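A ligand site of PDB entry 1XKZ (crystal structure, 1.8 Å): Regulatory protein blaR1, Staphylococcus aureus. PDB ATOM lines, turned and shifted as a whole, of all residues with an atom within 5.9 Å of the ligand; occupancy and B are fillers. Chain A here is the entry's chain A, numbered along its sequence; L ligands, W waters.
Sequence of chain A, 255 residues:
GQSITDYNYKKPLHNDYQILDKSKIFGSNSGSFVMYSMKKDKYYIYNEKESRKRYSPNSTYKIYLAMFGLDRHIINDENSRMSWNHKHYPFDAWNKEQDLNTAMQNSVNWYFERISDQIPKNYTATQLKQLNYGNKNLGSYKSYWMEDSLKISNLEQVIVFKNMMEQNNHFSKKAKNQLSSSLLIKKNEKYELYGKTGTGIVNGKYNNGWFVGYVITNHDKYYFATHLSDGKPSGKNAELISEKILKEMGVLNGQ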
ATOM      1  N   PRO A  57      25.180   8.246  13.404  1.00  0.00           N
ATOM      2  CA  PRO A  57      24.029   8.559  12.562  1.00  0.00           C
ATOM      3  C   PRO A  57      22.710   8.659  13.327  1.00  0.00           C
ATOM      4  O   PRO A  57      21.759   9.240  12.818  1.00  0.00           O
ATOM      5  CB  PRO A  57      23.983   7.364  11.617  1.00  0.00           C
ATOM      6  CG  PRO A  57      24.457   6.228  12.448  1.00  0.00           C
ATOM      7  CD  PRO A  57      25.577   6.845  13.227  1.00  0.00           C
ATOM      8  N   ASN A  58      22.635   8.334  14.546  1.00  0.00           N
ATOM      9  CA  ASN A  58      21.542   7.999  15.452  1.00  0.00           C
ATOM     10  C   ASN A  58      20.285   7.575  14.622  1.00  0.00           C
ATOM     11  O   ASN A  58      20.300   6.566  13.913  1.00  0.00           O
ATOM     12  CB  ASN A  58      21.211   9.184  16.423  1.00  0.00           C
ATOM     13  CG  ASN A  58      21.312  10.594  15.837  1.00  0.00           C
ATOM     14  OD1 ASN A  58      20.515  10.961  14.993  1.00  0.00           O
ATOM     15  ND2 ASN A  58      22.256  11.420  16.264  1.00  0.00           N
ATOM     16  N   SER A  59      19.117   8.297  14.666  1.00  0.00           N
ATOM     17  CA  SER A  59      17.890   7.896  13.934  1.00  0.00           C
ATOM     18  C   SER A  59      18.017   7.896  12.365  1.00  0.00           C
ATOM     19  O   SER A  59      17.176   7.307  11.676  1.00  0.00           O
ATOM     20  CB  SER A  59      16.729   8.778  14.331  1.00  0.00           C
ATOM     21  OG  SER A  59      16.457   8.546  15.704  1.00  0.00           O
ATOM     22  N   THR A  60      19.049   8.584  11.763  1.00  0.00           N
ATOM     23  CA  THR A  60      19.111   8.523  10.247  1.00  0.00           C
ATOM     24  C   THR A  60      19.505   7.115   9.807  1.00  0.00           C
ATOM     25  O   THR A  60      19.158   6.656   8.717  1.00  0.00           O
ATOM     26  CB  THR A  60      20.131   9.494   9.673  1.00  0.00           C
ATOM     27  OG1 THR A  60      21.435   9.136  10.118  1.00  0.00           O
ATOM     28  CG2 THR A  60      19.837  10.927  10.087  1.00  0.00           C
ATOM     29  N   LYS A  62      17.858   4.572  10.701  1.00  0.00           N
ATOM     30  CA  LYS A  62      16.553   3.904  10.525  1.00  0.00           C
ATOM     31  C   LYS A  62      16.294   3.694   9.043  1.00  0.00           C
ATOM     32  O   LYS A  62      15.634   2.728   8.641  1.00  0.00           O
ATOM     33  CB  LYS A  62      15.418   4.689  11.176  1.00  0.00           C
ATOM     34  CG  LYS A  62      15.544   4.667  12.731  1.00  0.00           C
ATOM     35  CD  LYS A  62      14.561   5.595  13.429  1.00  0.00           C
ATOM     36  CE  LYS A  62      14.761   5.391  14.919  1.00  0.00           C
ATOM     37  NZ  LYS A  62      13.834   6.182  15.657  1.00  0.00           N
ATOM     38  N   PHE A  91       7.030   9.444  24.538  1.00  0.00           N
ATOM     39  CA  PHE A  91       6.353  10.110  23.424  1.00  0.00           C
ATOM     40  C   PHE A  91       5.057   9.400  23.114  1.00  0.00           C
ATOM     41  O   PHE A  91       5.034   8.188  22.905  1.00  0.00           O
ATOM     42  CB  PHE A  91       7.221  10.096  22.172  1.00  0.00           C
ATOM     43  CG  PHE A  91       8.558  10.707  22.373  1.00  0.00           C
ATOM     44  CD1 PHE A  91       9.676   9.899  22.638  1.00  0.00           C
ATOM     45  CD2 PHE A  91       8.700  12.105  22.288  1.00  0.00           C
ATOM     46  CE1 PHE A  91      10.959  10.471  22.808  1.00  0.00           C
ATOM     47  CE2 PHE A  91       9.963  12.704  22.457  1.00  0.00           C
ATOM     48  CZ  PHE A  91      11.107  11.877  22.722  1.00  0.00           C
ATOM     49  N   TRP A  94       4.620   6.912  20.189  1.00  0.00           N
ATOM     50  CA  TRP A  94       5.260   5.604  20.257  1.00  0.00           C
ATOM     51  C   TRP A  94       4.370   4.563  20.963  1.00  0.00           C
ATOM     52  O   TRP A  94       4.640   3.348  20.877  1.00  0.00           O
ATOM     53  CB  TRP A  94       6.561   5.709  21.045  1.00  0.00           C
ATOM     54  CG  TRP A  94       7.648   6.553  20.415  1.00  0.00           C
ATOM     55  CD1 TRP A  94       7.560   7.417  19.353  1.00  0.00           C
ATOM     56  CD2 TRP A  94       9.019   6.563  20.824  1.00  0.00           C
ATOM     57  NE1 TRP A  94       8.799   7.984  19.084  1.00  0.00           N
ATOM     58  CE2 TRP A  94       9.706   7.479  19.973  1.00  0.00           C
ATOM     59  CE3 TRP A  94       9.735   5.872  21.819  1.00  0.00           C
ATOM     60  CZ2 TRP A  94      11.102   7.719  20.100  1.00  0.00           C
ATOM     61  CZ3 TRP A  94      11.117   6.110  21.949  1.00  0.00           C
ATOM     62  CH2 TRP A  94      11.786   7.026  21.083  1.00  0.00           C
ATOM     63  N   SER A 107       9.681   8.652  14.305  1.00  0.00           N
ATOM     64  CA  SER A 107      10.970   8.143  14.735  1.00  0.00           C
ATOM     65  C   SER A 107      10.801   7.219  15.959  1.00  0.00           C
ATOM     66  O   SER A 107      11.346   7.460  17.037  1.00  0.00           O
ATOM     67  CB  SER A 107      11.994   9.269  15.020  1.00  0.00           C
ATOM     68  OG  SER A 107      13.352   8.825  14.756  1.00  0.00           O
ATOM     69  N   ASN A 109      11.767   4.584  18.030  1.00  0.00           N
ATOM     70  CA  ASN A 109      12.939   3.746  18.254  1.00  0.00           C
ATOM     71  C   ASN A 109      12.686   2.260  18.392  1.00  0.00           C
ATOM     72  O   ASN A 109      13.375   1.451  17.753  1.00  0.00           O
ATOM     73  CB  ASN A 109      13.728   4.185  19.507  1.00  0.00           C
ATOM     74  CG  ASN A 109      14.420   5.540  19.371  1.00  0.00           C
ATOM     75  OD1 ASN A 109      14.430   6.198  18.318  1.00  0.00           O
ATOM     76  ND2 ASN A 109      14.970   6.005  20.497  1.00  0.00           N
ATOM     77  N   MET A 146      23.312   4.140  17.922  1.00  0.00           N
ATOM     78  CA  MET A 146      22.890   5.154  18.887  1.00  0.00           C
ATOM     79  C   MET A 146      24.015   5.738  19.744  1.00  0.00           C
ATOM     80  O   MET A 146      24.191   5.364  20.926  1.00  0.00           O
ATOM     81  CB  MET A 146      21.770   4.603  19.773  1.00  0.00           C
ATOM     82  CG  MET A 146      20.503   4.261  18.956  1.00  0.00           C
ATOM     83  SD  MET A 146      19.583   5.733  18.288  1.00  0.00           S
ATOM     84  CE  MET A 146      18.039   5.554  19.251  1.00  0.00           C
ATOM     85  N   GLU A 147      24.638   6.814  19.226  1.00  0.00           N
ATOM     86  CA  GLU A 147      25.761   7.518  19.879  1.00  0.00           C
ATOM     87  C   GLU A 147      26.762   6.536  20.450  1.00  0.00           C
ATOM     88  O   GLU A 147      27.136   6.563  21.635  1.00  0.00           O
ATOM     89  CB  GLU A 147      25.288   8.551  20.914  1.00  0.00           C
ATOM     90  CG  GLU A 147      24.354   9.621  20.346  1.00  0.00           C
ATOM     91  CD  GLU A 147      24.966  10.615  19.348  1.00  0.00           C
ATOM     92  OE1 GLU A 147      26.206  10.913  19.402  1.00  0.00           O
ATOM     93  OE2 GLU A 147      24.148  11.112  18.537  1.00  0.00           O
ATOM     94  N   LYS A 196      14.843  12.085   6.642  1.00  0.00           N
ATOM     95  CA  LYS A 196      14.746  11.527   7.985  1.00  0.00           C
ATOM     96  C   LYS A 196      15.594  12.368   8.946  1.00  0.00           C
ATOM     97  O   LYS A 196      16.740  12.630   8.655  1.00  0.00           O
ATOM     98  CB  LYS A 196      15.305  10.088   7.997  1.00  0.00           C
ATOM     99  CG  LYS A 196      15.302   9.391   9.379  1.00  0.00           C
ATOM    100  CD  LYS A 196      13.813   9.214   9.802  1.00  0.00           C
ATOM    101  CE  LYS A 196      13.681   8.688  11.233  1.00  0.00           C
ATOM    102  NZ  LYS A 196      13.842   9.864  12.205  1.00  0.00           N
ATOM    103  N   THR A 197      14.981  12.792  10.060  1.00  0.00           N
ATOM    104  CA  THR A 197      15.750  13.510  11.091  1.00  0.00           C
ATOM    105  C   THR A 197      16.526  12.548  12.023  1.00  0.00           C
ATOM    106  O   THR A 197      16.216  11.363  12.174  1.00  0.00           O
ATOM    107  CB  THR A 197      14.833  14.331  11.966  1.00  0.00           C
ATOM    108  OG1 THR A 197      13.735  13.500  12.370  1.00  0.00           O
ATOM    109  CG2 THR A 197      14.339  15.514  11.231  1.00  0.00           C
ATOM    110  N   GLY A 198      17.488  13.139  12.751  1.00  0.00           N
ATOM    111  CA  GLY A 198      18.242  12.408  13.750  1.00  0.00           C
ATOM    112  C   GLY A 198      18.601  13.415  14.853  1.00  0.00           C
ATOM    113  O   GLY A 198      18.925  14.576  14.549  1.00  0.00           O
ATOM    114  N   THR A 199      18.454  12.996  16.103  1.00  0.00           N
ATOM    115  CA  THR A 199      18.777  13.860  17.251  1.00  0.00           C
ATOM    116  C   THR A 199      19.443  13.037  18.306  1.00  0.00           C
ATOM    117  O   THR A 199      18.886  12.028  18.730  1.00  0.00           O
ATOM    118  CB  THR A 199      17.511  14.482  17.919  1.00  0.00           C
ATOM    119  OG1 THR A 199      16.722  15.180  16.957  1.00  0.00           O
ATOM    120  CG2 THR A 199      17.925  15.499  19.007  1.00  0.00           C
ATOM    121  N   GLY A 200      20.619  13.489  18.776  1.00  0.00           N
ATOM    122  CA  GLY A 200      21.335  12.789  19.821  1.00  0.00           C
ATOM    123  C   GLY A 200      21.429  13.642  21.077  1.00  0.00           C
ATOM    124  O   GLY A 200      21.314  14.878  20.983  1.00  0.00           O
ATOM    125  N   ILE A 201      21.396  13.011  22.256  1.00  0.00           N
ATOM    126  CA  ILE A 201      21.540  13.778  23.507  1.00  0.00           C
ATOM    127  C   ILE A 201      22.546  13.081  24.416  1.00  0.00           C
ATOM    128  O   ILE A 201      22.510  11.851  24.617  1.00  0.00           O
ATOM    129  CB  ILE A 201      20.195  14.031  24.246  1.00  0.00           C
ATOM    130  CG1 ILE A 201      20.417  14.995  25.415  1.00  0.00           C
ATOM    131  CG2 ILE A 201      19.597  12.711  24.726  1.00  0.00           C
ATOM    132  CD1 ILE A 201      19.138  15.585  26.041  1.00  0.00           C
ATOM    133  N   VAL A 202      23.461  13.886  24.943  1.00  0.00           N
ATOM    134  CA  VAL A 202      24.519  13.406  25.801  1.00  0.00           C
ATOM    135  C   VAL A 202      24.723  14.509  26.857  1.00  0.00           C
ATOM    136  O   VAL A 202      24.544  15.713  26.558  1.00  0.00           O
ATOM    137  CB  VAL A 202      25.775  13.172  24.965  1.00  0.00           C
ATOM    138  N   TYR A 206      21.750  18.670  23.538  1.00  0.00           N
ATOM    139  CA  TYR A 206      21.653  18.202  22.133  1.00  0.00           C
ATOM    140  C   TYR A 206      23.085  18.289  21.632  1.00  0.00           C
ATOM    141  O   TYR A 206      23.727  19.336  21.797  1.00  0.00           O
ATOM    142  CB  TYR A 206      20.777  19.121  21.298  1.00  0.00           C
ATOM    143  CG  TYR A 206      19.272  19.010  21.482  1.00  0.00           C
ATOM    144  CD1 TYR A 206      18.454  20.142  21.328  1.00  0.00           C
ATOM    145  CD2 TYR A 206      18.650  17.764  21.758  1.00  0.00           C
ATOM    146  CE1 TYR A 206      17.026  20.055  21.430  1.00  0.00           C
ATOM    147  CE2 TYR A 206      17.216  17.658  21.879  1.00  0.00           C
ATOM    148  CZ  TYR A 206      16.417  18.812  21.702  1.00  0.00           C
ATOM    149  OH  TYR A 206      15.042  18.722  21.777  1.00  0.00           O
ATOM    150  N   ASN A 207      23.598  17.214  21.021  1.00  0.00           N
ATOM    151  CA  ASN A 207      24.983  17.229  20.577  1.00  0.00           C
ATOM    152  C   ASN A 207      25.254  16.788  19.120  1.00  0.00           C
ATOM    153  O   ASN A 207      26.366  16.994  18.612  1.00  0.00           O
ATOM    154  CB  ASN A 207      25.803  16.324  21.546  1.00  0.00           C
ATOM    155  CG  ASN A 207      25.579  14.810  21.304  1.00  0.00           C
ATOM    156  OD1 ASN A 207      24.462  14.385  21.073  1.00  0.00           O
ATOM    157  ND2 ASN A 207      26.653  14.022  21.280  1.00  0.00           N
ATOM    158  N   TRP A 210      20.723  15.781  12.686  1.00  0.00           N
ATOM    159  CA  TRP A 210      20.799  15.423  11.276  1.00  0.00           C
ATOM    160  C   TRP A 210      19.475  15.537  10.543  1.00  0.00           C
ATOM    161  O   TRP A 210      18.377  15.526  11.146  1.00  0.00           O
ATOM    162  CB  TRP A 210      21.052  13.914  11.074  1.00  0.00           C
ATOM    163  CG  TRP A 210      22.282  13.290  11.539  1.00  0.00           C
ATOM    164  CD1 TRP A 210      22.465  12.562  12.685  1.00  0.00           C
ATOM    165  CD2 TRP A 210      23.510  13.221  10.816  1.00  0.00           C
ATOM    166  NE1 TRP A 210      23.755  12.044  12.726  1.00  0.00           N
ATOM    167  CE2 TRP A 210      24.410  12.426  11.575  1.00  0.00           C
ATOM    168  CE3 TRP A 210      23.946  13.768   9.593  1.00  0.00           C
ATOM    169  CZ2 TRP A 210      25.732  12.132  11.163  1.00  0.00           C
ATOM    170  CZ3 TRP A 210      25.263  13.488   9.173  1.00  0.00           C
ATOM    171  CH2 TRP A 210      26.136  12.678   9.960  1.00  0.00           C
ATOM    172  N   SER A 234      19.581  19.936  16.923  1.00  0.00           N
ATOM    173  CA  SER A 234      18.502  18.959  16.915  1.00  0.00           C
ATOM    174  C   SER A 234      18.168  18.609  15.478  1.00  0.00           C
ATOM    175  O   SER A 234      18.433  19.406  14.578  1.00  0.00           O
ATOM    176  CB  SER A 234      17.268  19.568  17.551  1.00  0.00           C
ATOM    177  OG  SER A 234      16.837  20.720  16.836  1.00  0.00           O
ATOM    178  N   GLY A 235      17.549  17.457  15.272  1.00  0.00           N
ATOM    179  CA  GLY A 235      17.129  17.080  13.941  1.00  0.00           C
ATOM    180  C   GLY A 235      16.110  18.064  13.387  1.00  0.00           C
ATOM    181  O   GLY A 235      16.109  18.334  12.183  1.00  0.00           O
ATOM    182  N   LYS A 236      15.271  18.632  14.280  1.00  0.00           N
ATOM    183  CA  LYS A 236      14.255  19.616  13.903  1.00  0.00           C
ATOM    184  C   LYS A 236      14.908  20.861  13.303  1.00  0.00           C
ATOM    185  O   LYS A 236      14.440  21.360  12.275  1.00  0.00           O
ATOM    186  CB  LYS A 236      13.411  20.021  15.166  1.00  0.00           C
HETATM  187  S1  LIG L   1      13.854  10.080  19.301  1.00  0.00           S
HETATM  188  C1  LIG L   1      14.224  11.776  19.428  1.00  0.00           C
HETATM  189  C2  LIG L   1      14.125  12.624  18.232  1.00  0.00           C
HETATM  190  C3  LIG L   1      13.804  13.918  18.373  1.00  0.00           C
HETATM  191  C4  LIG L   1      14.407  12.065  16.935  1.00  0.00           C
HETATM  192  C5  LIG L   1      14.406  12.777  15.546  1.00  0.00           C
HETATM  193  O1  LIG L   1      13.736  12.217  14.600  1.00  0.00           O
HETATM  194  O2  LIG L   1      15.072  13.857  15.435  1.00  0.00           O
HETATM  195  N1  LIG L   1      14.743  10.614  16.801  1.00  0.00           N
HETATM  196  C6  LIG L   1      14.761   9.653  17.870  1.00  0.00           C
HETATM  197  C7  LIG L   1      16.161   9.162  18.008  1.00  0.00           C
HETATM  198  C8  LIG L   1      16.913   9.249  16.667  1.00  0.00           C
HETATM  199  O3  LIG L   1      17.680  10.173  16.444  1.00  0.00           O
HETATM  200  N2  LIG L   1      17.020   9.912  19.007  1.00  0.00           N
HETATM  201  C9  LIG L   1      17.178   9.435  20.275  1.00  0.00           C
HETATM  202  O4  LIG L   1      16.639   8.422  20.651  1.00  0.00           O
HETATM  203  C10 LIG L   1      18.079  10.158  21.163  1.00  0.00           C
HETATM  204  N3  LIG L   1      17.851  11.262  21.915  1.00  0.00           N
HETATM  205  O5  LIG L   1      16.482  11.769  21.791  1.00  0.00           O
HETATM  206  C11 LIG L   1      16.012  12.608  22.905  1.00  0.00           C
HETATM  207  C12 LIG L   1      19.408   9.604  21.409  1.00  0.00           C
HETATM  208  C13 LIG L   1      19.880   8.385  20.802  1.00  0.00           C
HETATM  209  S2  LIG L   1      21.400   7.901  21.305  1.00  0.00           S
HETATM  210  C14 LIG L   1      21.481   9.296  22.287  1.00  0.00           C
HETATM  211  N4  LIG L   1      22.577   9.601  23.107  1.00  0.00           N
HETATM  212  N5  LIG L   1      20.414  10.048  22.231  1.00  0.00           N
HETATM  213  C15 LIG L   1      14.502  12.717  22.719  1.00  0.00           C
HETATM  214  C16 LIG L   1      16.646  14.017  22.751  1.00  0.00           C
HETATM  215  C17 LIG L   1      16.219  12.039  24.378  1.00  0.00           C
HETATM  216  O6  LIG L   1      16.262  12.894  25.365  1.00  0.00           O
HETATM  217  O7  LIG L   1      16.301  10.761  24.571  1.00  0.00           O
HETATM  218  O   HOH W   1      14.800   8.937  23.225  1.00  0.00           O
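N of Ser 59 lies close to O3 of the ligand, at 3.0 Å.
The side-chain hydroxyl of Ser 59 is covalently linked to a carbon (C8) of the ligand (1.3 Å).
O1 of the ligand is in hydrogen-bond range of OG1 of Thr 197 (2.6 Å).
N of Thr 199 is in hydrogen-bond range of O3 of the ligand, 2.9 Å away.
A nitrogen (N2) of the ligand sits at hydrogen-bond distance from the backbone carbonyl oxygen of Thr 199, 2.8 Å away.
The side-chain hydroxyl (OG1) of Thr 199 sits at hydrogen-bond distance from an oxygen (O2) of the ligand (2.6 Å).
N5 of the ligand is in hydrogen-bond range of N of Ile 201, at 3.1 Å.
A nitrogen (N4) of the ligand sits at hydrogen-bond distance from the backbone carbonyl oxygen (O) of Ile 201.
The side-chain amide nitrogen (ND2) of Asn 109 lies within hydrogen-bond range of an oxygen (O4) of the ligand, at 2.9 Å.
OG of Ser 107 is in hydrogen-bond range of N1 of the ligand.
An oxygen (O3) of the ligand sits close to the side-chain amide oxygen of Asn 58.
An oxygen (O1) of the ligand lies within salt-bridge range of the side-chain amino group (NZ) of Lys 196.
OG of Ser 107 lies within hydrogen-bond range of OG of Ser 59 (3.3 Å).
The side-chain amino group of Lys 196 sits at hydrogen-bond distance from the side-chain hydroxyl of Ser 107.
The backbone carbonyl oxygen of Ser 107 sits close to the indole nitrogen of Trp 94.
OG of Ser 107 sits at hydrogen-bond distance from NZ of Lys 62, at 2.8 Å.
The side-chain carboxylate (OE2) of Glu 147 sits at hydrogen-bond distance from the side-chain amide nitrogen (ND2) of Asn 58, 3.0 Å away.
N of Gly 235 sits close to O of Gly 198 (3.3 Å).
The backbone carbonyl oxygen of Gly 198 is in hydrogen-bond range of the backbone NH of Trp 210, 2.9 Å away.
The side-chain amide oxygen (OD1) of Asn 207 lies close to the backbone carbonyl oxygen (O) of Gly 200 (3.2 Å).
A sulfur (S2) of the ligand lies close to the backbone carbonyl oxygen (O) of Met 146, 3.8 Å away.
Merely in contact with the ligand: Glu 147, Phe 91, Gly 198, Trp 94, Gly 200 and Tyr 206.
Hydrophobic or aromatic side chains within 4 Å of the ligand: Phe 91, Trp 94, Met 146, Ile 201 and Tyr 206.
15 residues have an atom within 4 Å of the ligand: Asn 58, Ser 59, Phe 91, Trp 94, Ser 107, Asn 109, Met 146, Glu 147, Lys 196, Thr 197, Gly 198, Thr 199, Gly 200, Ile 201 and Tyr 206.
The nearest printed residue that does not touch the ligand is Gly 235 (4.1 Å).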
